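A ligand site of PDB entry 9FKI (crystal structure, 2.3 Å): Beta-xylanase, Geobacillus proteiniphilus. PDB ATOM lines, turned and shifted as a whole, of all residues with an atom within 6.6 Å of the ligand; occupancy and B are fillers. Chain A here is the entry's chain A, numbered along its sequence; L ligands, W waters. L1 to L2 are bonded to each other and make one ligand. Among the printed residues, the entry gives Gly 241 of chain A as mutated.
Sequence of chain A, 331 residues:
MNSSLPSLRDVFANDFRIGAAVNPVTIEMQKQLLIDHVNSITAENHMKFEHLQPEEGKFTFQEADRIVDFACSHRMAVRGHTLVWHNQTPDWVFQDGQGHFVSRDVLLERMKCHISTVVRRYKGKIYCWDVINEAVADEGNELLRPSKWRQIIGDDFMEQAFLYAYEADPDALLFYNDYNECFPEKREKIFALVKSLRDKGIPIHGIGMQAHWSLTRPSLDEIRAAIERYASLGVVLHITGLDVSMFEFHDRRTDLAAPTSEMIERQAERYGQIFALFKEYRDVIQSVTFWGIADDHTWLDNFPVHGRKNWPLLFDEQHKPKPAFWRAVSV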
ATOM      1  N   ALA A  43      30.379  -6.062 -22.614  1.00  0.00           N
ATOM      2  CA  ALA A  43      31.497  -6.971 -22.827  1.00  0.00           C
ATOM      3  C   ALA A  43      31.082  -8.036 -23.832  1.00  0.00           C
ATOM      4  O   ALA A  43      30.138  -8.784 -23.602  1.00  0.00           O
ATOM      5  CB  ALA A  43      31.935  -7.622 -21.509  1.00  0.00           C
ATOM      6  N   GLU A  44      31.819  -8.110 -24.948  1.00  0.00           N
ATOM      7  CA  GLU A  44      31.500  -9.093 -25.970  1.00  0.00           C
ATOM      8  C   GLU A  44      31.683 -10.515 -25.454  1.00  0.00           C
ATOM      9  O   GLU A  44      30.935 -11.422 -25.834  1.00  0.00           O
ATOM     10  CB  GLU A  44      32.394  -8.871 -27.204  1.00  0.00           C
ATOM     11  CG  GLU A  44      31.956  -9.687 -28.425  1.00  0.00           C
ATOM     12  CD  GLU A  44      32.886  -9.517 -29.606  1.00  0.00           C
ATOM     13  OE1 GLU A  44      33.795  -8.667 -29.517  1.00  0.00           O
ATOM     14  OE2 GLU A  44      32.703 -10.214 -30.615  1.00  0.00           O
ATOM     15  N   ASN A  45      32.690 -10.752 -24.603  1.00  0.00           N
ATOM     16  CA  ASN A  45      32.928 -12.098 -24.103  1.00  0.00           C
ATOM     17  C   ASN A  45      33.348 -12.158 -22.638  1.00  0.00           C
ATOM     18  O   ASN A  45      33.119 -13.194 -22.012  1.00  0.00           O
ATOM     19  CB  ASN A  45      34.003 -12.801 -24.942  1.00  0.00           C
ATOM     20  CG  ASN A  45      33.471 -13.329 -26.255  1.00  0.00           C
ATOM     21  OD1 ASN A  45      32.586 -14.188 -26.269  1.00  0.00           O
ATOM     22  ND2 ASN A  45      33.986 -12.808 -27.363  1.00  0.00           N
ATOM     23  N   LYS A  48      31.106 -13.402 -19.648  1.00  0.00           N
ATOM     24  CA  LYS A  48      30.472 -14.709 -19.692  1.00  0.00           C
ATOM     25  C   LYS A  48      31.096 -15.626 -18.641  1.00  0.00           C
ATOM     26  O   LYS A  48      32.217 -15.401 -18.170  1.00  0.00           O
ATOM     27  CB  LYS A  48      30.577 -15.309 -21.080  1.00  0.00           C
ATOM     28  CG  LYS A  48      29.831 -14.469 -22.130  1.00  0.00           C
ATOM     29  CD  LYS A  48      30.294 -14.760 -23.530  1.00  0.00           C
ATOM     30  CE  LYS A  48      29.479 -13.988 -24.558  1.00  0.00           C
ATOM     31  NZ  LYS A  48      29.827 -14.429 -25.940  1.00  0.00           N
ATOM     32  N   HIS A  81      26.653  -8.885 -19.473  1.00  0.00           N
ATOM     33  CA  HIS A  81      26.352  -9.992 -20.381  1.00  0.00           C
ATOM     34  C   HIS A  81      27.378 -11.098 -20.152  1.00  0.00           C
ATOM     35  O   HIS A  81      28.564 -10.868 -20.420  1.00  0.00           O
ATOM     36  CB  HIS A  81      26.387  -9.521 -21.839  1.00  0.00           C
ATOM     37  CG  HIS A  81      26.066 -10.581 -22.843  1.00  0.00           C
ATOM     38  ND1 HIS A  81      24.781 -10.901 -23.203  1.00  0.00           N
ATOM     39  CD2 HIS A  81      26.876 -11.396 -23.566  1.00  0.00           C
ATOM     40  CE1 HIS A  81      24.795 -11.867 -24.102  1.00  0.00           C
ATOM     41  NE2 HIS A  81      26.054 -12.190 -24.341  1.00  0.00           N
ATOM     42  N   THR A  82      26.966 -12.293 -19.710  1.00  0.00           N
ATOM     43  CA  THR A  82      25.613 -12.709 -19.339  1.00  0.00           C
ATOM     44  C   THR A  82      25.778 -13.800 -18.264  1.00  0.00           C
ATOM     45  O   THR A  82      26.812 -14.454 -18.199  1.00  0.00           O
ATOM     46  CB  THR A  82      24.799 -13.274 -20.544  1.00  0.00           C
ATOM     47  OG1 THR A  82      23.539 -13.732 -20.077  1.00  0.00           O
ATOM     48  CG2 THR A  82      25.514 -14.455 -21.189  1.00  0.00           C
ATOM     49  N   TRP A  85      23.637 -19.168 -19.435  1.00  0.00           N
ATOM     50  CA  TRP A  85      23.586 -19.412 -20.876  1.00  0.00           C
ATOM     51  C   TRP A  85      24.025 -20.846 -21.148  1.00  0.00           C
ATOM     52  O   TRP A  85      24.885 -21.385 -20.437  1.00  0.00           O
ATOM     53  CB  TRP A  85      24.531 -18.450 -21.620  1.00  0.00           C
ATOM     54  CG  TRP A  85      24.440 -18.433 -23.135  1.00  0.00           C
ATOM     55  CD1 TRP A  85      23.374 -18.839 -23.904  1.00  0.00           C
ATOM     56  CD2 TRP A  85      25.436 -17.951 -24.049  1.00  0.00           C
ATOM     57  NE1 TRP A  85      23.662 -18.641 -25.236  1.00  0.00           N
ATOM     58  CE2 TRP A  85      24.907 -18.092 -25.354  1.00  0.00           C
ATOM     59  CE3 TRP A  85      26.706 -17.398 -23.896  1.00  0.00           C
ATOM     60  CZ2 TRP A  85      25.631 -17.720 -26.496  1.00  0.00           C
ATOM     61  CZ3 TRP A  85      27.421 -17.029 -25.036  1.00  0.00           C
ATOM     62  CH2 TRP A  85      26.876 -17.176 -26.316  1.00  0.00           C
ATOM     63  N   GLN A  88      29.446 -21.180 -23.577  1.00  0.00           N
ATOM     64  CA  GLN A  88      30.561 -20.554 -22.891  1.00  0.00           C
ATOM     65  C   GLN A  88      30.442 -20.675 -21.376  1.00  0.00           C
ATOM     66  O   GLN A  88      30.717 -19.717 -20.650  1.00  0.00           O
ATOM     67  CB  GLN A  88      30.683 -19.094 -23.354  1.00  0.00           C
ATOM     68  CG  GLN A  88      31.115 -19.022 -24.827  1.00  0.00           C
ATOM     69  CD  GLN A  88      31.314 -17.616 -25.337  1.00  0.00           C
ATOM     70  OE1 GLN A  88      30.428 -17.027 -25.962  1.00  0.00           O
ATOM     71  NE2 GLN A  88      32.499 -17.053 -25.079  1.00  0.00           N
ATOM     72  N   ASP A 130      21.857  -9.157 -18.562  1.00  0.00           N
ATOM     73  CA  ASP A 130      21.239 -10.266 -19.292  1.00  0.00           C
ATOM     74  C   ASP A 130      21.342 -11.500 -18.404  1.00  0.00           C
ATOM     75  O   ASP A 130      22.345 -12.225 -18.439  1.00  0.00           O
ATOM     76  CB  ASP A 130      21.926 -10.504 -20.641  1.00  0.00           C
ATOM     77  CG  ASP A 130      21.820  -9.315 -21.584  1.00  0.00           C
ATOM     78  OD1 ASP A 130      20.831  -8.551 -21.513  1.00  0.00           O
ATOM     79  OD2 ASP A 130      22.726  -9.162 -22.450  1.00  0.00           O
ATOM     80  N   ASN A 133      20.174 -16.078 -21.169  1.00  0.00           N
ATOM     81  CA  ASN A 133      20.501 -15.868 -22.574  1.00  0.00           C
ATOM     82  C   ASN A 133      19.991 -17.067 -23.374  1.00  0.00           C
ATOM     83  O   ASN A 133      20.381 -18.206 -23.104  1.00  0.00           O
ATOM     84  CB  ASN A 133      22.003 -15.685 -22.777  1.00  0.00           C
ATOM     85  CG  ASN A 133      22.337 -14.866 -24.044  1.00  0.00           C
ATOM     86  OD1 ASN A 133      21.657 -13.894 -24.365  1.00  0.00           O
ATOM     87  ND2 ASN A 133      23.403 -15.247 -24.738  1.00  0.00           N
ATOM     88  N   GLU A 134      19.090 -16.804 -24.325  1.00  0.00           N
ATOM     89  CA  GLU A 134      18.770 -17.750 -25.412  1.00  0.00           C
ATOM     90  C   GLU A 134      18.199 -19.072 -24.899  1.00  0.00           C
ATOM     91  O   GLU A 134      18.559 -20.135 -25.410  1.00  0.00           O
ATOM     92  CB  GLU A 134      19.998 -18.019 -26.273  1.00  0.00           C
ATOM     93  CG  GLU A 134      20.537 -16.789 -26.944  1.00  0.00           C
ATOM     94  CD  GLU A 134      21.879 -17.027 -27.599  1.00  0.00           C
ATOM     95  OE1 GLU A 134      22.489 -16.032 -28.047  1.00  0.00           O
ATOM     96  OE2 GLU A 134      22.318 -18.201 -27.670  1.00  0.00           O
ATOM     97  N   ASN A 177      17.295 -12.256 -22.835  1.00  0.00           N
ATOM     98  CA  ASN A 177      17.991 -11.805 -24.055  1.00  0.00           C
ATOM     99  C   ASN A 177      18.027 -12.946 -25.087  1.00  0.00           C
ATOM    100  O   ASN A 177      18.380 -14.077 -24.754  1.00  0.00           O
ATOM    101  CB  ASN A 177      19.417 -11.340 -23.698  1.00  0.00           C
ATOM    102  CG  ASN A 177      20.134 -10.619 -24.847  1.00  0.00           C
ATOM    103  OD1 ASN A 177      19.696  -9.563 -25.292  1.00  0.00           O
ATOM    104  ND2 ASN A 177      21.244 -11.184 -25.314  1.00  0.00           N
ATOM    105  N   TYR A 179      17.884 -14.035 -29.705  1.00  0.00           N
ATOM    106  CA  TYR A 179      18.052 -13.744 -31.128  1.00  0.00           C
ATOM    107  C   TYR A 179      16.972 -14.454 -31.926  1.00  0.00           C
ATOM    108  O   TYR A 179      16.230 -15.290 -31.400  1.00  0.00           O
ATOM    109  CB  TYR A 179      19.445 -14.152 -31.621  1.00  0.00           C
ATOM    110  CG  TYR A 179      19.643 -15.654 -31.653  1.00  0.00           C
ATOM    111  CD1 TYR A 179      20.021 -16.353 -30.505  1.00  0.00           C
ATOM    112  CD2 TYR A 179      19.395 -16.381 -32.820  1.00  0.00           C
ATOM    113  CE1 TYR A 179      20.190 -17.747 -30.540  1.00  0.00           C
ATOM    114  CE2 TYR A 179      19.552 -17.770 -32.858  1.00  0.00           C
ATOM    115  CZ  TYR A 179      19.954 -18.446 -31.710  1.00  0.00           C
ATOM    116  OH  TYR A 179      20.103 -19.814 -31.749  1.00  0.00           O
ATOM    117  N   GLN A 210      18.383  -9.190 -29.656  1.00  0.00           N
ATOM    118  CA  GLN A 210      19.759  -9.190 -30.154  1.00  0.00           C
ATOM    119  C   GLN A 210      19.875  -8.517 -31.512  1.00  0.00           C
ATOM    120  O   GLN A 210      20.842  -7.781 -31.757  1.00  0.00           O
ATOM    121  CB  GLN A 210      20.311 -10.618 -30.219  1.00  0.00           C
ATOM    122  CG  GLN A 210      20.742 -11.205 -28.867  1.00  0.00           C
ATOM    123  CD  GLN A 210      21.319 -12.601 -28.982  1.00  0.00           C
ATOM    124  OE1 GLN A 210      21.866 -12.980 -30.012  1.00  0.00           O
ATOM    125  NE2 GLN A 210      21.159 -13.390 -27.927  1.00  0.00           N
ATOM    126  N   HIS A 212      20.485  -9.822 -34.587  1.00  0.00           N
ATOM    127  CA  HIS A 212      21.507 -10.289 -35.511  1.00  0.00           C
ATOM    128  C   HIS A 212      20.781 -10.516 -36.836  1.00  0.00           C
ATOM    129  O   HIS A 212      20.318 -11.624 -37.138  1.00  0.00           O
ATOM    130  CB  HIS A 212      22.236 -11.530 -34.985  1.00  0.00           C
ATOM    131  CG  HIS A 212      23.124 -11.243 -33.809  1.00  0.00           C
ATOM    132  ND1 HIS A 212      24.118 -10.284 -33.832  1.00  0.00           N
ATOM    133  CD2 HIS A 212      23.144 -11.769 -32.557  1.00  0.00           C
ATOM    134  CE1 HIS A 212      24.718 -10.242 -32.651  1.00  0.00           C
ATOM    135  NE2 HIS A 212      24.152 -11.139 -31.866  1.00  0.00           N
ATOM    136  N   THR A 240      20.214  -5.335 -28.275  1.00  0.00           N
ATOM    137  CA  THR A 240      21.435  -5.621 -27.546  1.00  0.00           C
ATOM    138  C   THR A 240      22.639  -6.026 -28.391  1.00  0.00           C
ATOM    139  O   THR A 240      23.764  -5.871 -27.916  1.00  0.00           O
ATOM    140  CB  THR A 240      21.202  -6.721 -26.509  1.00  0.00           C
ATOM    141  OG1 THR A 240      20.651  -7.871 -27.168  1.00  0.00           O
ATOM    142  CG2 THR A 240      20.239  -6.235 -25.422  1.00  0.00           C
ATOM    143  N   GLY A 241      22.442  -6.527 -29.610  1.00  0.00           N
ATOM    144  CA  GLY A 241      23.579  -6.994 -30.402  1.00  0.00           C
ATOM    145  C   GLY A 241      23.474  -6.683 -31.884  1.00  0.00           C
ATOM    146  O   GLY A 241      23.876  -7.485 -32.727  1.00  0.00           O
ATOM    147  N   TRP A 291      26.694  -5.036 -31.924  1.00  0.00           N
ATOM    148  CA  TRP A 291      27.669  -6.047 -31.510  1.00  0.00           C
ATOM    149  C   TRP A 291      29.038  -5.786 -32.149  1.00  0.00           C
ATOM    150  O   TRP A 291      29.573  -6.597 -32.912  1.00  0.00           O
ATOM    151  CB  TRP A 291      27.160  -7.447 -31.816  1.00  0.00           C
ATOM    152  CG  TRP A 291      27.652  -8.469 -30.829  1.00  0.00           C
ATOM    153  CD1 TRP A 291      28.427  -9.578 -31.089  1.00  0.00           C
ATOM    154  CD2 TRP A 291      27.408  -8.488 -29.409  1.00  0.00           C
ATOM    155  NE1 TRP A 291      28.659 -10.282 -29.923  1.00  0.00           N
ATOM    156  CE2 TRP A 291      28.049  -9.632 -28.884  1.00  0.00           C
ATOM    157  CE3 TRP A 291      26.695  -7.645 -28.536  1.00  0.00           C
ATOM    158  CZ2 TRP A 291      28.015  -9.957 -27.515  1.00  0.00           C
ATOM    159  CZ3 TRP A 291      26.657  -7.967 -27.181  1.00  0.00           C
ATOM    160  CH2 TRP A 291      27.309  -9.121 -26.684  1.00  0.00           C
ATOM    161  N   HIS A 297      36.397  -5.184 -36.701  1.00  0.00           N
ATOM    162  CA  HIS A 297      36.167  -6.266 -35.742  1.00  0.00           C
ATOM    163  C   HIS A 297      34.689  -6.624 -35.739  1.00  0.00           C
ATOM    164  O   HIS A 297      33.855  -5.809 -35.346  1.00  0.00           O
ATOM    165  CB  HIS A 297      36.591  -5.875 -34.327  1.00  0.00           C
ATOM    166  CG  HIS A 297      36.285  -6.926 -33.298  1.00  0.00           C
ATOM    167  ND1 HIS A 297      37.098  -8.018 -33.098  1.00  0.00           N
ATOM    168  CD2 HIS A 297      35.233  -7.069 -32.456  1.00  0.00           C
ATOM    169  CE1 HIS A 297      36.571  -8.779 -32.146  1.00  0.00           C
ATOM    170  NE2 HIS A 297      35.444  -8.221 -31.743  1.00  0.00           N
ATOM    171  N   THR A 298      34.385  -7.857 -36.147  1.00  0.00           N
ATOM    172  CA  THR A 298      33.043  -8.403 -36.035  1.00  0.00           C
ATOM    173  C   THR A 298      33.119  -9.927 -35.925  1.00  0.00           C
ATOM    174  O   THR A 298      33.890 -10.576 -36.650  1.00  0.00           O
ATOM    175  CB  THR A 298      32.156  -8.000 -37.209  1.00  0.00           C
ATOM    176  OG1 THR A 298      30.910  -8.712 -37.139  1.00  0.00           O
ATOM    177  CG2 THR A 298      32.833  -8.319 -38.537  1.00  0.00           C
ATOM    178  N   TRP A 299      32.305 -10.478 -35.032  1.00  0.00           N
ATOM    179  CA  TRP A 299      32.173 -11.920 -34.898  1.00  0.00           C
ATOM    180  C   TRP A 299      31.615 -12.565 -36.160  1.00  0.00           C
ATOM    181  O   TRP A 299      31.759 -13.786 -36.324  1.00  0.00           O
ATOM    182  CB  TRP A 299      31.280 -12.247 -33.698  1.00  0.00           C
ATOM    183  CG  TRP A 299      29.813 -11.979 -33.941  1.00  0.00           C
ATOM    184  CD1 TRP A 299      29.234 -10.786 -34.274  1.00  0.00           C
ATOM    185  CD2 TRP A 299      28.750 -12.928 -33.848  1.00  0.00           C
ATOM    186  NE1 TRP A 299      27.858 -10.944 -34.408  1.00  0.00           N
ATOM    187  CE2 TRP A 299      27.548 -12.253 -34.138  1.00  0.00           C
ATOM    188  CE3 TRP A 299      28.699 -14.291 -33.547  1.00  0.00           C
ATOM    189  CZ2 TRP A 299      26.318 -12.893 -34.152  1.00  0.00           C
ATOM    190  CZ3 TRP A 299      27.481 -14.931 -33.549  1.00  0.00           C
ATOM    191  CH2 TRP A 299      26.304 -14.242 -33.856  1.00  0.00           C
HETATM  192  C1  LIG L   1      24.736 -13.053 -29.199  1.00  0.00           C
HETATM  193  C2  LIG L   1      25.214 -13.709 -27.921  1.00  0.00           C
HETATM  194  C3  LIG L   1      26.623 -13.181 -27.678  1.00  0.00           C
HETATM  195  C4  LIG L   1      27.480 -13.744 -28.797  1.00  0.00           C
HETATM  196  C5  LIG L   1      26.920 -13.276 -30.149  1.00  0.00           C
HETATM  197  O1  LIG L   1      24.314 -13.490 -26.835  1.00  0.00           O
HETATM  198  O2  LIG L   1      27.127 -13.586 -26.410  1.00  0.00           O
HETATM  199  O3  LIG L   1      28.801 -13.236 -28.696  1.00  0.00           O
HETATM  200  O4  LIG L   1      25.521 -13.575 -30.275  1.00  0.00           O
HETATM  201  F1  LIG L   1      24.807 -11.658 -29.129  1.00  0.00           F
HETATM  202  C1  LG2 L   2      29.619 -13.891 -29.643  1.00  0.00           C
HETATM  203  C2  LG2 L   2      31.001 -13.266 -29.579  1.00  0.00           C
HETATM  204  C3  LG2 L   2      32.034 -14.227 -30.144  1.00  0.00           C
HETATM  205  C4  LG2 L   2      32.080 -15.492 -29.288  1.00  0.00           C
HETATM  206  C5  LG2 L   2      30.692 -15.938 -28.789  1.00  0.00           C
HETATM  207  O1  LG2 L   2      30.997 -12.046 -30.329  1.00  0.00           O
HETATM  208  O2  LG2 L   2      33.287 -13.531 -30.137  1.00  0.00           O
HETATM  209  O3  LG2 L   2      32.746 -16.573 -29.956  1.00  0.00           O
HETATM  210  O4  LG2 L   2      29.589 -15.319 -29.431  1.00  0.00           O
HETATM  211  O   HOH W   1      24.488 -16.103 -30.307  1.00  0.00           O
HETATM  212  O   HOH W   2      23.287  -9.725 -26.895  1.00  0.00           O
HETATM  213  O   HOH W   3      31.495 -17.451 -32.777  1.00  0.00           O
HETATM  214  O   HOH W   4      34.194 -19.237 -30.513  1.00  0.00           O
HETATM  215  O   HOH W   5      29.091 -18.749 -27.946  1.00  0.00           O
HETATM  216  O   HOH W   6      34.585 -11.552 -32.116  1.00  0.00           O
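The side-chain carboxylate (OE2) of Glu 44 is in hydrogen-bond range of an oxygen (O1) of LG2 L2, 2.5 Å away. An oxygen (O2) of LIG L1 sits at hydrogen-bond distance from a ring nitrogen (NE2) of His 81 (2.7 Å). NE2 of His 212 sits at hydrogen-bond distance from O4 of LIG L1 (3.2 Å). An oxygen (O2) of LIG L1 lies within hydrogen-bond range of the side-chain amino group of Lys 48 (2.9 Å). ND2 of Asn 133 is in hydrogen-bond range of O1 of LIG L1 (2.9 Å). The side-chain amide nitrogen (ND2) of Asn 45 lies within hydrogen-bond range of an oxygen (O2) of LG2 L2. The indole nitrogen (NE1) of Trp 291 sits at hydrogen-bond distance from an oxygen (O1) of LG2 L2 (3.0 Å). An oxygen (O1) of LIG L1 is in hydrogen-bond range of the side-chain amide nitrogen of Gln 210 (3.3 Å). OE1 of Glu 134 lies within hydrogen-bond range of O1 of LIG L1 (3.4 Å).
The side-chain amino group (NZ) of Lys 48 is in hydrogen-bond range of the backbone carbonyl oxygen (O) of Glu 44 (3.2 Å). A ring nitrogen (NE2) of His 212 lies close to the side-chain amide oxygen (OE1) of Gln 210, 3.5 Å away. A ring nitrogen (ND1) of His 212 lies close to the backbone carbonyl oxygen (O) of Gly 241. The side-chain amide oxygen (OD1) of Asn 45 lies within hydrogen-bond range of the side-chain amino group (NZ) of Lys 48, 2.8 Å away. The side-chain amide oxygen (OD1) of Asn 133 sits at hydrogen-bond distance from the side-chain amide nitrogen (ND2) of Asn 177 (2.9 Å). The side-chain amide nitrogen (NE2) of Gln 210 sits close to the side-chain amide nitrogen (ND2) of Asn 177. OE2 of Glu 134 lies within hydrogen-bond range of NE1 of Trp 85 (2.8 Å). The backbone carbonyl oxygen (O) of Asn 177 lies within hydrogen-bond range of the backbone NH (N) of Glu 134, 2.9 Å away.
Merely in contact with the ligand: Trp 85 (3.6 Å), Gln 88 (3.0 Å) and Trp 299 (3.4 Å). 12 residues have an atom within 4 Å of the ligand: Glu 44, Asn 45, Lys 48, His 81, Trp 85, Gln 88, Asn 133, Glu 134, Gln 210, His 212, Trp 291 and Trp 299. Along chain A the residues within 4 Å of the ligand span positions 44 to 299.
Water W1 bridges O4 of LIG L1 (2.7 Å) and OE1 of Glu 134 (3.0 Å). Water W6 lies within hydrogen-bond range of the side-chain carboxylate (OE2) of Glu 44, an oxygen (O2) of LG2 L2 and a ring nitrogen (NE2) of His 297. Water W2 bridges the side-chain amide nitrogen (ND2) of Asn 177 (3.0 Å) and the side-chain hydroxyl (OG1) of Thr 240 (3.2 Å).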
